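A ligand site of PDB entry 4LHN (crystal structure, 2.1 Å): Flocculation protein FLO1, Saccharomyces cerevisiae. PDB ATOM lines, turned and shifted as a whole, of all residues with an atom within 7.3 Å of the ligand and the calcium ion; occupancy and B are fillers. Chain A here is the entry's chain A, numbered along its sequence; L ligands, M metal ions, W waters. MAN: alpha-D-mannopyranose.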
ATOM      1  N   SER A  29      -0.428  19.351   0.646  1.00  0.00           N
ATOM      2  CA  SER A  29       0.451  19.940  -0.328  1.00  0.00           C
ATOM      3  C   SER A  29       0.251  19.380  -1.753  1.00  0.00           C
ATOM      4  O   SER A  29       1.129  19.517  -2.520  1.00  0.00           O
ATOM      5  CB  SER A  29       1.879  19.724   0.106  1.00  0.00           C
ATOM      6  OG  SER A  29       2.104  18.329   0.057  1.00  0.00           O
ATOM      7  N   TYR A  32      -4.093  21.632  -3.936  1.00  0.00           N
ATOM      8  CA  TYR A  32      -4.031  23.048  -4.276  1.00  0.00           C
ATOM      9  C   TYR A  32      -3.360  23.285  -5.658  1.00  0.00           C
ATOM     10  O   TYR A  32      -3.580  24.316  -6.289  1.00  0.00           O
ATOM     11  CB  TYR A  32      -3.282  23.854  -3.157  1.00  0.00           C
ATOM     12  CG  TYR A  32      -1.763  23.833  -3.258  1.00  0.00           C
ATOM     13  CD1 TYR A  32      -1.007  22.751  -2.823  1.00  0.00           C
ATOM     14  CD2 TYR A  32      -1.090  24.905  -3.840  1.00  0.00           C
ATOM     15  CE1 TYR A  32       0.343  22.746  -2.932  1.00  0.00           C
ATOM     16  CE2 TYR A  32       0.250  24.913  -3.982  1.00  0.00           C
ATOM     17  CZ  TYR A  32       0.968  23.842  -3.515  1.00  0.00           C
ATOM     18  OH  TYR A  32       2.302  23.882  -3.663  1.00  0.00           O
ATOM     19  N   TYR A  61      -3.375  37.528   4.387  1.00  0.00           N
ATOM     20  CA  TYR A  61      -3.535  36.922   5.681  1.00  0.00           C
ATOM     21  C   TYR A  61      -2.169  36.568   6.268  1.00  0.00           C
ATOM     22  O   TYR A  61      -1.341  35.972   5.628  1.00  0.00           O
ATOM     23  CB  TYR A  61      -4.365  35.617   5.583  1.00  0.00           C
ATOM     24  CG  TYR A  61      -4.376  34.882   6.873  1.00  0.00           C
ATOM     25  CD1 TYR A  61      -5.014  35.426   7.971  1.00  0.00           C
ATOM     26  CD2 TYR A  61      -3.644  33.720   7.045  1.00  0.00           C
ATOM     27  CE1 TYR A  61      -4.986  34.820   9.199  1.00  0.00           C
ATOM     28  CE2 TYR A  61      -3.641  33.035   8.276  1.00  0.00           C
ATOM     29  CZ  TYR A  61      -4.266  33.594   9.346  1.00  0.00           C
ATOM     30  OH  TYR A  61      -4.245  33.001  10.578  1.00  0.00           O
ATOM     31  N   GLN A  76       4.909  38.174   6.588  1.00  0.00           N
ATOM     32  CA  GLN A  76       5.710  37.020   6.264  1.00  0.00           C
ATOM     33  C   GLN A  76       7.142  37.401   6.080  1.00  0.00           C
ATOM     34  O   GLN A  76       8.020  36.680   6.486  1.00  0.00           O
ATOM     35  CB  GLN A  76       5.190  36.315   4.989  1.00  0.00           C
ATOM     36  CG  GLN A  76       5.953  35.012   4.736  1.00  0.00           C
ATOM     37  CD  GLN A  76       5.340  34.031   3.716  1.00  0.00           C
ATOM     38  OE1 GLN A  76       4.392  34.322   2.961  1.00  0.00           O
ATOM     39  NE2 GLN A  76       5.901  32.841   3.695  1.00  0.00           N
ATOM     40  N   GLN A  95       3.648  27.532  13.463  1.00  0.00           N
ATOM     41  CA  GLN A  95       3.210  27.935  12.154  1.00  0.00           C
ATOM     42  C   GLN A  95       2.356  26.896  11.426  1.00  0.00           C
ATOM     43  O   GLN A  95       1.726  27.211  10.401  1.00  0.00           O
ATOM     44  CB  GLN A  95       4.382  28.285  11.242  1.00  0.00           C
ATOM     45  CG  GLN A  95       5.407  29.283  11.694  1.00  0.00           C
ATOM     46  CD  GLN A  95       6.453  29.541  10.574  1.00  0.00           C
ATOM     47  OE1 GLN A  95       6.501  28.873   9.534  1.00  0.00           O
ATOM     48  NE2 GLN A  95       7.241  30.538  10.769  1.00  0.00           N
ATOM     49  N   PRO A 111      -8.367  30.789   7.967  1.00  0.00           N
ATOM     50  CA  PRO A 111      -7.743  31.307   6.748  1.00  0.00           C
ATOM     51  C   PRO A 111      -6.429  30.656   6.400  1.00  0.00           C
ATOM     52  O   PRO A 111      -5.977  30.809   5.270  1.00  0.00           O
ATOM     53  CB  PRO A 111      -7.567  32.796   7.026  1.00  0.00           C
ATOM     54  CG  PRO A 111      -8.252  33.075   8.314  1.00  0.00           C
ATOM     55  CD  PRO A 111      -8.280  31.783   9.056  1.00  0.00           C
ATOM     56  N   THR A 112      -5.836  29.913   7.357  1.00  0.00           N
ATOM     57  CA  THR A 112      -4.682  29.048   7.113  1.00  0.00           C
ATOM     58  C   THR A 112      -4.880  27.913   6.111  1.00  0.00           C
ATOM     59  O   THR A 112      -3.941  27.423   5.576  1.00  0.00           O
ATOM     60  CB  THR A 112      -4.269  28.331   8.411  1.00  0.00           C
ATOM     61  OG1 THR A 112      -5.415  27.766   9.075  1.00  0.00           O
ATOM     62  CG2 THR A 112      -3.605  29.308   9.341  1.00  0.00           C
ATOM     63  N   ASP A 138       0.224  32.899  -2.698  1.00  0.00           N
ATOM     64  CA  ASP A 138       0.453  31.912  -1.662  1.00  0.00           C
ATOM     65  C   ASP A 138      -0.936  31.393  -1.177  1.00  0.00           C
ATOM     66  O   ASP A 138      -1.645  32.146  -0.551  1.00  0.00           O
ATOM     67  CB  ASP A 138       1.277  32.540  -0.536  1.00  0.00           C
ATOM     68  CG  ASP A 138       1.647  31.558   0.583  1.00  0.00           C
ATOM     69  OD1 ASP A 138       1.032  30.456   0.699  1.00  0.00           O
ATOM     70  OD2 ASP A 138       2.560  31.903   1.361  1.00  0.00           O
ATOM     71  N   ASP A 139      -1.355  30.177  -1.513  1.00  0.00           N
ATOM     72  CA  ASP A 139      -0.601  29.117  -2.220  1.00  0.00           C
ATOM     73  C   ASP A 139      -0.893  28.907  -3.701  1.00  0.00           C
ATOM     74  O   ASP A 139       0.011  28.533  -4.455  1.00  0.00           O
ATOM     75  CB  ASP A 139      -0.864  27.793  -1.498  1.00  0.00           C
ATOM     76  CG  ASP A 139      -0.115  27.685  -0.144  1.00  0.00           C
ATOM     77  OD1 ASP A 139       1.110  27.428  -0.238  1.00  0.00           O
ATOM     78  OD2 ASP A 139      -0.690  27.920   0.936  1.00  0.00           O
ATOM     79  N   SER A 140      -2.142  29.069  -4.115  1.00  0.00           N
ATOM     80  CA  SER A 140      -2.515  28.913  -5.539  1.00  0.00           C
ATOM     81  C   SER A 140      -3.778  29.686  -5.845  1.00  0.00           C
ATOM     82  O   SER A 140      -4.593  29.918  -4.939  1.00  0.00           O
ATOM     83  CB  SER A 140      -2.663  27.457  -5.956  1.00  0.00           C
ATOM     84  OG  SER A 140      -3.803  26.938  -5.350  1.00  0.00           O
ATOM     85  N   LYS A 172       2.494  28.659  -5.875  1.00  0.00           N
ATOM     86  CA  LYS A 172       3.733  28.718  -5.096  1.00  0.00           C
ATOM     87  C   LYS A 172       4.225  27.261  -4.931  1.00  0.00           C
ATOM     88  O   LYS A 172       3.486  26.411  -4.400  1.00  0.00           O
ATOM     89  CB  LYS A 172       3.494  29.406  -3.751  1.00  0.00           C
ATOM     90  CG  LYS A 172       4.626  29.386  -2.710  1.00  0.00           C
ATOM     91  CD  LYS A 172       4.107  30.010  -1.434  1.00  0.00           C
ATOM     92  CE  LYS A 172       5.240  30.457  -0.516  1.00  0.00           C
ATOM     93  NZ  LYS A 172       6.082  29.307  -0.038  1.00  0.00           N
ATOM     94  N   PRO A 173       5.457  26.955  -5.412  1.00  0.00           N
ATOM     95  CA  PRO A 173       5.918  25.540  -5.217  1.00  0.00           C
ATOM     96  C   PRO A 173       6.053  25.306  -3.704  1.00  0.00           C
ATOM     97  O   PRO A 173       6.333  26.253  -2.942  1.00  0.00           O
ATOM     98  CB  PRO A 173       7.275  25.472  -5.937  1.00  0.00           C
ATOM     99  CG  PRO A 173       7.679  26.913  -6.243  1.00  0.00           C
ATOM    100  CD  PRO A 173       6.523  27.858  -5.915  1.00  0.00           C
ATOM    101  N   TRP A 174       5.831  24.074  -3.265  1.00  0.00           N
ATOM    102  CA  TRP A 174       5.722  23.792  -1.847  1.00  0.00           C
ATOM    103  C   TRP A 174       7.047  24.013  -1.183  1.00  0.00           C
ATOM    104  O   TRP A 174       7.977  23.344  -1.474  1.00  0.00           O
ATOM    105  CB  TRP A 174       5.334  22.350  -1.618  1.00  0.00           C
ATOM    106  CG  TRP A 174       4.987  22.105  -0.234  1.00  0.00           C
ATOM    107  CD1 TRP A 174       5.738  21.550   0.703  1.00  0.00           C
ATOM    108  CD2 TRP A 174       3.784  22.487   0.397  1.00  0.00           C
ATOM    109  NE1 TRP A 174       5.091  21.512   1.880  1.00  0.00           N
ATOM    110  CE2 TRP A 174       3.880  22.108   1.725  1.00  0.00           C
ATOM    111  CE3 TRP A 174       2.619  23.102  -0.035  1.00  0.00           C
ATOM    112  CZ2 TRP A 174       2.867  22.302   2.610  1.00  0.00           C
ATOM    113  CZ3 TRP A 174       1.628  23.298   0.854  1.00  0.00           C
ATOM    114  CH2 TRP A 174       1.762  22.907   2.151  1.00  0.00           C
ATOM    115  N   GLY A 175       7.106  24.984  -0.306  1.00  0.00           N
ATOM    116  CA  GLY A 175       8.285  25.339   0.429  1.00  0.00           C
ATOM    117  C   GLY A 175       9.160  26.355  -0.279  1.00  0.00           C
ATOM    118  O   GLY A 175      10.070  26.911   0.316  1.00  0.00           O
ATOM    119  N   GLY A 176       8.823  26.623  -1.517  1.00  0.00           N
ATOM    120  CA  GLY A 176       9.511  27.564  -2.373  1.00  0.00           C
ATOM    121  C   GLY A 176       9.227  29.005  -2.038  1.00  0.00           C
ATOM    122  O   GLY A 176       8.364  29.305  -1.270  1.00  0.00           O
ATOM    123  N   SER A 177       9.996  29.900  -2.610  1.00  0.00           N
ATOM    124  CA  SER A 177       9.741  31.306  -2.434  1.00  0.00           C
ATOM    125  C   SER A 177       8.514  31.768  -3.246  1.00  0.00           C
ATOM    126  O   SER A 177       8.053  31.098  -4.113  1.00  0.00           O
ATOM    127  CB  SER A 177      10.989  32.116  -2.735  1.00  0.00           C
ATOM    128  OG  SER A 177      11.262  32.143  -4.099  1.00  0.00           O
ATOM    129  N   LEU A 178       7.985  32.909  -2.882  1.00  0.00           N
ATOM    130  CA  LEU A 178       6.828  33.433  -3.539  1.00  0.00           C
ATOM    131  C   LEU A 178       7.107  33.645  -5.013  1.00  0.00           C
ATOM    132  O   LEU A 178       8.169  34.069  -5.388  1.00  0.00           O
ATOM    133  CB  LEU A 178       6.415  34.721  -2.872  1.00  0.00           C
ATOM    134  CG  LEU A 178       5.948  34.576  -1.451  1.00  0.00           C
ATOM    135  CD1 LEU A 178       6.172  35.873  -0.737  1.00  0.00           C
ATOM    136  CD2 LEU A 178       4.508  34.154  -1.363  1.00  0.00           C
ATOM    137  N   TYR A 200      -9.047  30.675  -5.090  1.00  0.00           N
ATOM    138  CA  TYR A 200      -7.836  30.872  -4.299  1.00  0.00           C
ATOM    139  C   TYR A 200      -7.766  29.785  -3.231  1.00  0.00           C
ATOM    140  O   TYR A 200      -8.769  29.493  -2.649  1.00  0.00           O
ATOM    141  CB  TYR A 200      -7.866  32.271  -3.646  1.00  0.00           C
ATOM    142  CG  TYR A 200      -6.850  32.370  -2.544  1.00  0.00           C
ATOM    143  CD1 TYR A 200      -5.495  32.541  -2.815  1.00  0.00           C
ATOM    144  CD2 TYR A 200      -7.205  32.253  -1.241  1.00  0.00           C
ATOM    145  CE1 TYR A 200      -4.556  32.582  -1.790  1.00  0.00           C
ATOM    146  CE2 TYR A 200      -6.242  32.314  -0.210  1.00  0.00           C
ATOM    147  CZ  TYR A 200      -4.960  32.450  -0.489  1.00  0.00           C
ATOM    148  OH  TYR A 200      -4.047  32.451   0.517  1.00  0.00           O
ATOM    149  N   SER A 201      -6.614  29.179  -3.038  1.00  0.00           N
ATOM    150  CA  SER A 201      -6.358  28.256  -1.951  1.00  0.00           C
ATOM    151  C   SER A 201      -5.165  28.667  -1.081  1.00  0.00           C
ATOM    152  O   SER A 201      -4.142  29.063  -1.565  1.00  0.00           O
ATOM    153  CB  SER A 201      -6.142  26.817  -2.405  1.00  0.00           C
ATOM    154  OG  SER A 201      -7.146  26.301  -3.179  1.00  0.00           O
ATOM    155  N   ASN A 202      -5.357  28.522   0.213  1.00  0.00           N
ATOM    156  CA  ASN A 202      -4.314  28.531   1.196  1.00  0.00           C
ATOM    157  C   ASN A 202      -4.226  27.140   1.865  1.00  0.00           C
ATOM    158  O   ASN A 202      -5.190  26.626   2.297  1.00  0.00           O
ATOM    159  CB  ASN A 202      -4.499  29.638   2.214  1.00  0.00           C
ATOM    160  CG  ASN A 202      -3.261  29.879   3.068  1.00  0.00           C
ATOM    161  OD1 ASN A 202      -2.239  29.458   2.744  1.00  0.00           O
ATOM    162  ND2 ASN A 202      -3.401  30.574   4.131  1.00  0.00           N
ATOM    163  N   ALA A 203      -3.057  26.559   1.876  1.00  0.00           N
ATOM    164  CA  ALA A 203      -2.871  25.238   2.401  1.00  0.00           C
ATOM    165  C   ALA A 203      -2.295  25.228   3.816  1.00  0.00           C
ATOM    166  O   ALA A 203      -2.547  24.349   4.556  1.00  0.00           O
ATOM    167  CB  ALA A 203      -2.015  24.441   1.471  1.00  0.00           C
ATOM    168  N   VAL A 204      -1.497  26.227   4.151  1.00  0.00           N
ATOM    169  CA  VAL A 204      -0.954  26.414   5.489  1.00  0.00           C
ATOM    170  C   VAL A 204      -0.518  27.859   5.729  1.00  0.00           C
ATOM    171  O   VAL A 204      -0.113  28.496   4.850  1.00  0.00           O
ATOM    172  CB  VAL A 204       0.231  25.457   5.727  1.00  0.00           C
ATOM    173  CG1 VAL A 204       1.429  25.836   4.897  1.00  0.00           C
ATOM    174  CG2 VAL A 204       0.550  25.299   7.191  1.00  0.00           C
ATOM    175  N   SER A 205      -0.616  28.332   6.966  1.00  0.00           N
ATOM    176  CA  SER A 205      -0.006  29.607   7.379  1.00  0.00           C
ATOM    177  C   SER A 205      -0.359  30.800   6.485  1.00  0.00           C
ATOM    178  O   SER A 205      -1.500  31.049   6.288  1.00  0.00           O
ATOM    179  CB  SER A 205       1.481  29.508   7.775  1.00  0.00           C
ATOM    180  OG  SER A 205       2.334  29.220   6.688  1.00  0.00           O
ATOM    181  N   TRP A 206       0.596  31.550   5.971  1.00  0.00           N
ATOM    182  CA  TRP A 206       0.301  32.789   5.237  1.00  0.00           C
ATOM    183  C   TRP A 206      -0.533  32.620   3.944  1.00  0.00           C
ATOM    184  O   TRP A 206      -0.362  31.645   3.221  1.00  0.00           O
ATOM    185  CB  TRP A 206       1.601  33.540   4.921  1.00  0.00           C
ATOM    186  CG  TRP A 206       2.231  34.178   6.116  1.00  0.00           C
ATOM    187  CD1 TRP A 206       1.947  35.415   6.630  1.00  0.00           C
ATOM    188  CD2 TRP A 206       3.248  33.624   6.957  1.00  0.00           C
ATOM    189  NE1 TRP A 206       2.727  35.656   7.735  1.00  0.00           N
ATOM    190  CE2 TRP A 206       3.536  34.569   7.952  1.00  0.00           C
ATOM    191  CE3 TRP A 206       3.940  32.405   6.956  1.00  0.00           C
ATOM    192  CZ2 TRP A 206       4.485  34.354   8.944  1.00  0.00           C
ATOM    193  CZ3 TRP A 206       4.889  32.190   7.948  1.00  0.00           C
ATOM    194  CH2 TRP A 206       5.151  33.160   8.924  1.00  0.00           C
ATOM    195  N   GLY A 207      -1.405  33.582   3.676  1.00  0.00           N
ATOM    196  CA  GLY A 207      -2.149  33.634   2.434  1.00  0.00           C
ATOM    197  C   GLY A 207      -1.966  34.990   1.771  1.00  0.00           C
ATOM    198  O   GLY A 207      -2.104  36.019   2.426  1.00  0.00           O
ATOM    199  N   THR A 208      -1.654  34.997   0.483  1.00  0.00           N
ATOM    200  CA  THR A 208      -1.417  36.246  -0.227  1.00  0.00           C
ATOM    201  C   THR A 208      -1.911  36.150  -1.615  1.00  0.00           C
ATOM    202  O   THR A 208      -1.629  35.148  -2.277  1.00  0.00           O
ATOM    203  CB  THR A 208       0.102  36.565  -0.302  1.00  0.00           C
ATOM    204  OG1 THR A 208       0.650  36.448   1.038  1.00  0.00           O
ATOM    205  CG2 THR A 208       0.328  37.985  -0.702  1.00  0.00           C
HETATM  206  C1  MAN L   1       5.836  28.574   3.702  1.00  0.00           C
HETATM  207  C2  MAN L   1       4.847  29.747   3.677  1.00  0.00           C
HETATM  208  C3  MAN L   1       3.417  29.249   3.520  1.00  0.00           C
HETATM  209  C4  MAN L   1       3.303  28.252   2.369  1.00  0.00           C
HETATM  210  C5  MAN L   1       4.375  27.170   2.478  1.00  0.00           C
HETATM  211  C6  MAN L   1       4.313  26.219   1.290  1.00  0.00           C
HETATM  212  O1  MAN L   1       5.579  27.768   4.863  1.00  0.00           O
HETATM  213  O2  MAN L   1       5.169  30.613   2.590  1.00  0.00           O
HETATM  214  O3  MAN L   1       2.546  30.362   3.276  1.00  0.00           O
HETATM  215  O4  MAN L   1       2.009  27.636   2.396  1.00  0.00           O
HETATM  216  O5  MAN L   1       5.661  27.792   2.528  1.00  0.00           O
HETATM  217  O6  MAN L   1       4.795  26.881   0.115  1.00  0.00           O
HETATM  218 CA    CA M   1       0.171  29.486   2.583  1.00  0.00          CA
HETATM  219  O   HOH W   1       2.983  26.252  -1.688  1.00  0.00           O
HETATM  220  O   HOH W   2       4.961  28.655   7.361  1.00  0.00           O
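Five residues have an atom within 4 Å of the calcium ion: Asp 138, Asp 139, Asn 202, Val 204 and Trp 206. Along chain A the residues within 4 Å of the calcium ion span positions 138 to 206.
The backbone carbonyl oxygen (O) of Asp 139 is in hydrogen-bond range of the backbone NH (N) of Lys 172 (2.9 Å). ND2 of Asn 202 sits at hydrogen-bond distance from O of Ser 205 (2.9 Å). The backbone NH of Asp 138 sits at hydrogen-bond distance from the backbone carbonyl oxygen of Thr 208 (2.9 Å). O of Gly 176 sits at hydrogen-bond distance from NZ of Lys 172 (2.6 Å). ND2 of Asn 202 lies within hydrogen-bond range of O of Pro 111. OE1 of Gln 76 lies close to OD2 of Asp 138, 3.4 Å away. O of Asp 138 sits at hydrogen-bond distance from OH of Tyr 200 (2.6 Å). The backbone NH (N) of Asp 139 sits at hydrogen-bond distance from the backbone carbonyl oxygen (O) of Ser 201.
The calcium ion is bound by OD1 of Asp 138 (2.3 Å), O of Trp 206 (2.3 Å), OD1 of Asn 202 (2.4 Å), OD2 of Asp 139 (2.4 Å), O of Val 204 (2.5 Å), O4 of the ligand (2.6 Å) and O3 of the ligand (2.6 Å). The calcium ion has seven donor atoms within binding distance.
An oxygen (O6) of the ligand lies within hydrogen-bond range of the backbone carbonyl oxygen (O) of Pro 173, 3.5 Å away. The side-chain amino group (NZ) of Lys 172 sits at hydrogen-bond distance from an oxygen (O6) of the ligand (2.8 Å). O6 of the ligand is in hydrogen-bond range of N of Gly 175 (3.0 Å). The side-chain amide nitrogen (NE2) of Gln 76 is in hydrogen-bond range of an oxygen (O2) of the ligand.
Merely in contact with the ligand: Trp 174 (3.8 Å) and Ser 205 (3.3 Å). Hydrophobic or aromatic side chains that line the ligand: Trp 174, Val 204 and Trp 206. Within 4 Å of the ligand: Gln 76, Asp 138, Asp 139, Lys 172, Pro 173, Trp 174, Gly 175, Val 204, Ser 205 and Trp 206. The nearest printed residue that does not touch the ligand is Gly 176 (4.4 Å).
Water W1 lies within hydrogen-bond range of an oxygen (O6) of the ligand, the side-chain carboxylate of Asp 139, the backbone carbonyl oxygen of Lys 172 and the side-chain hydroxyl of Tyr 32. Water W2 lies within hydrogen-bond range of the side-chain amide oxygen (OE1) of Gln 95, an oxygen (O1) of the ligand and the side-chain hydroxyl (OG) of Ser 205.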
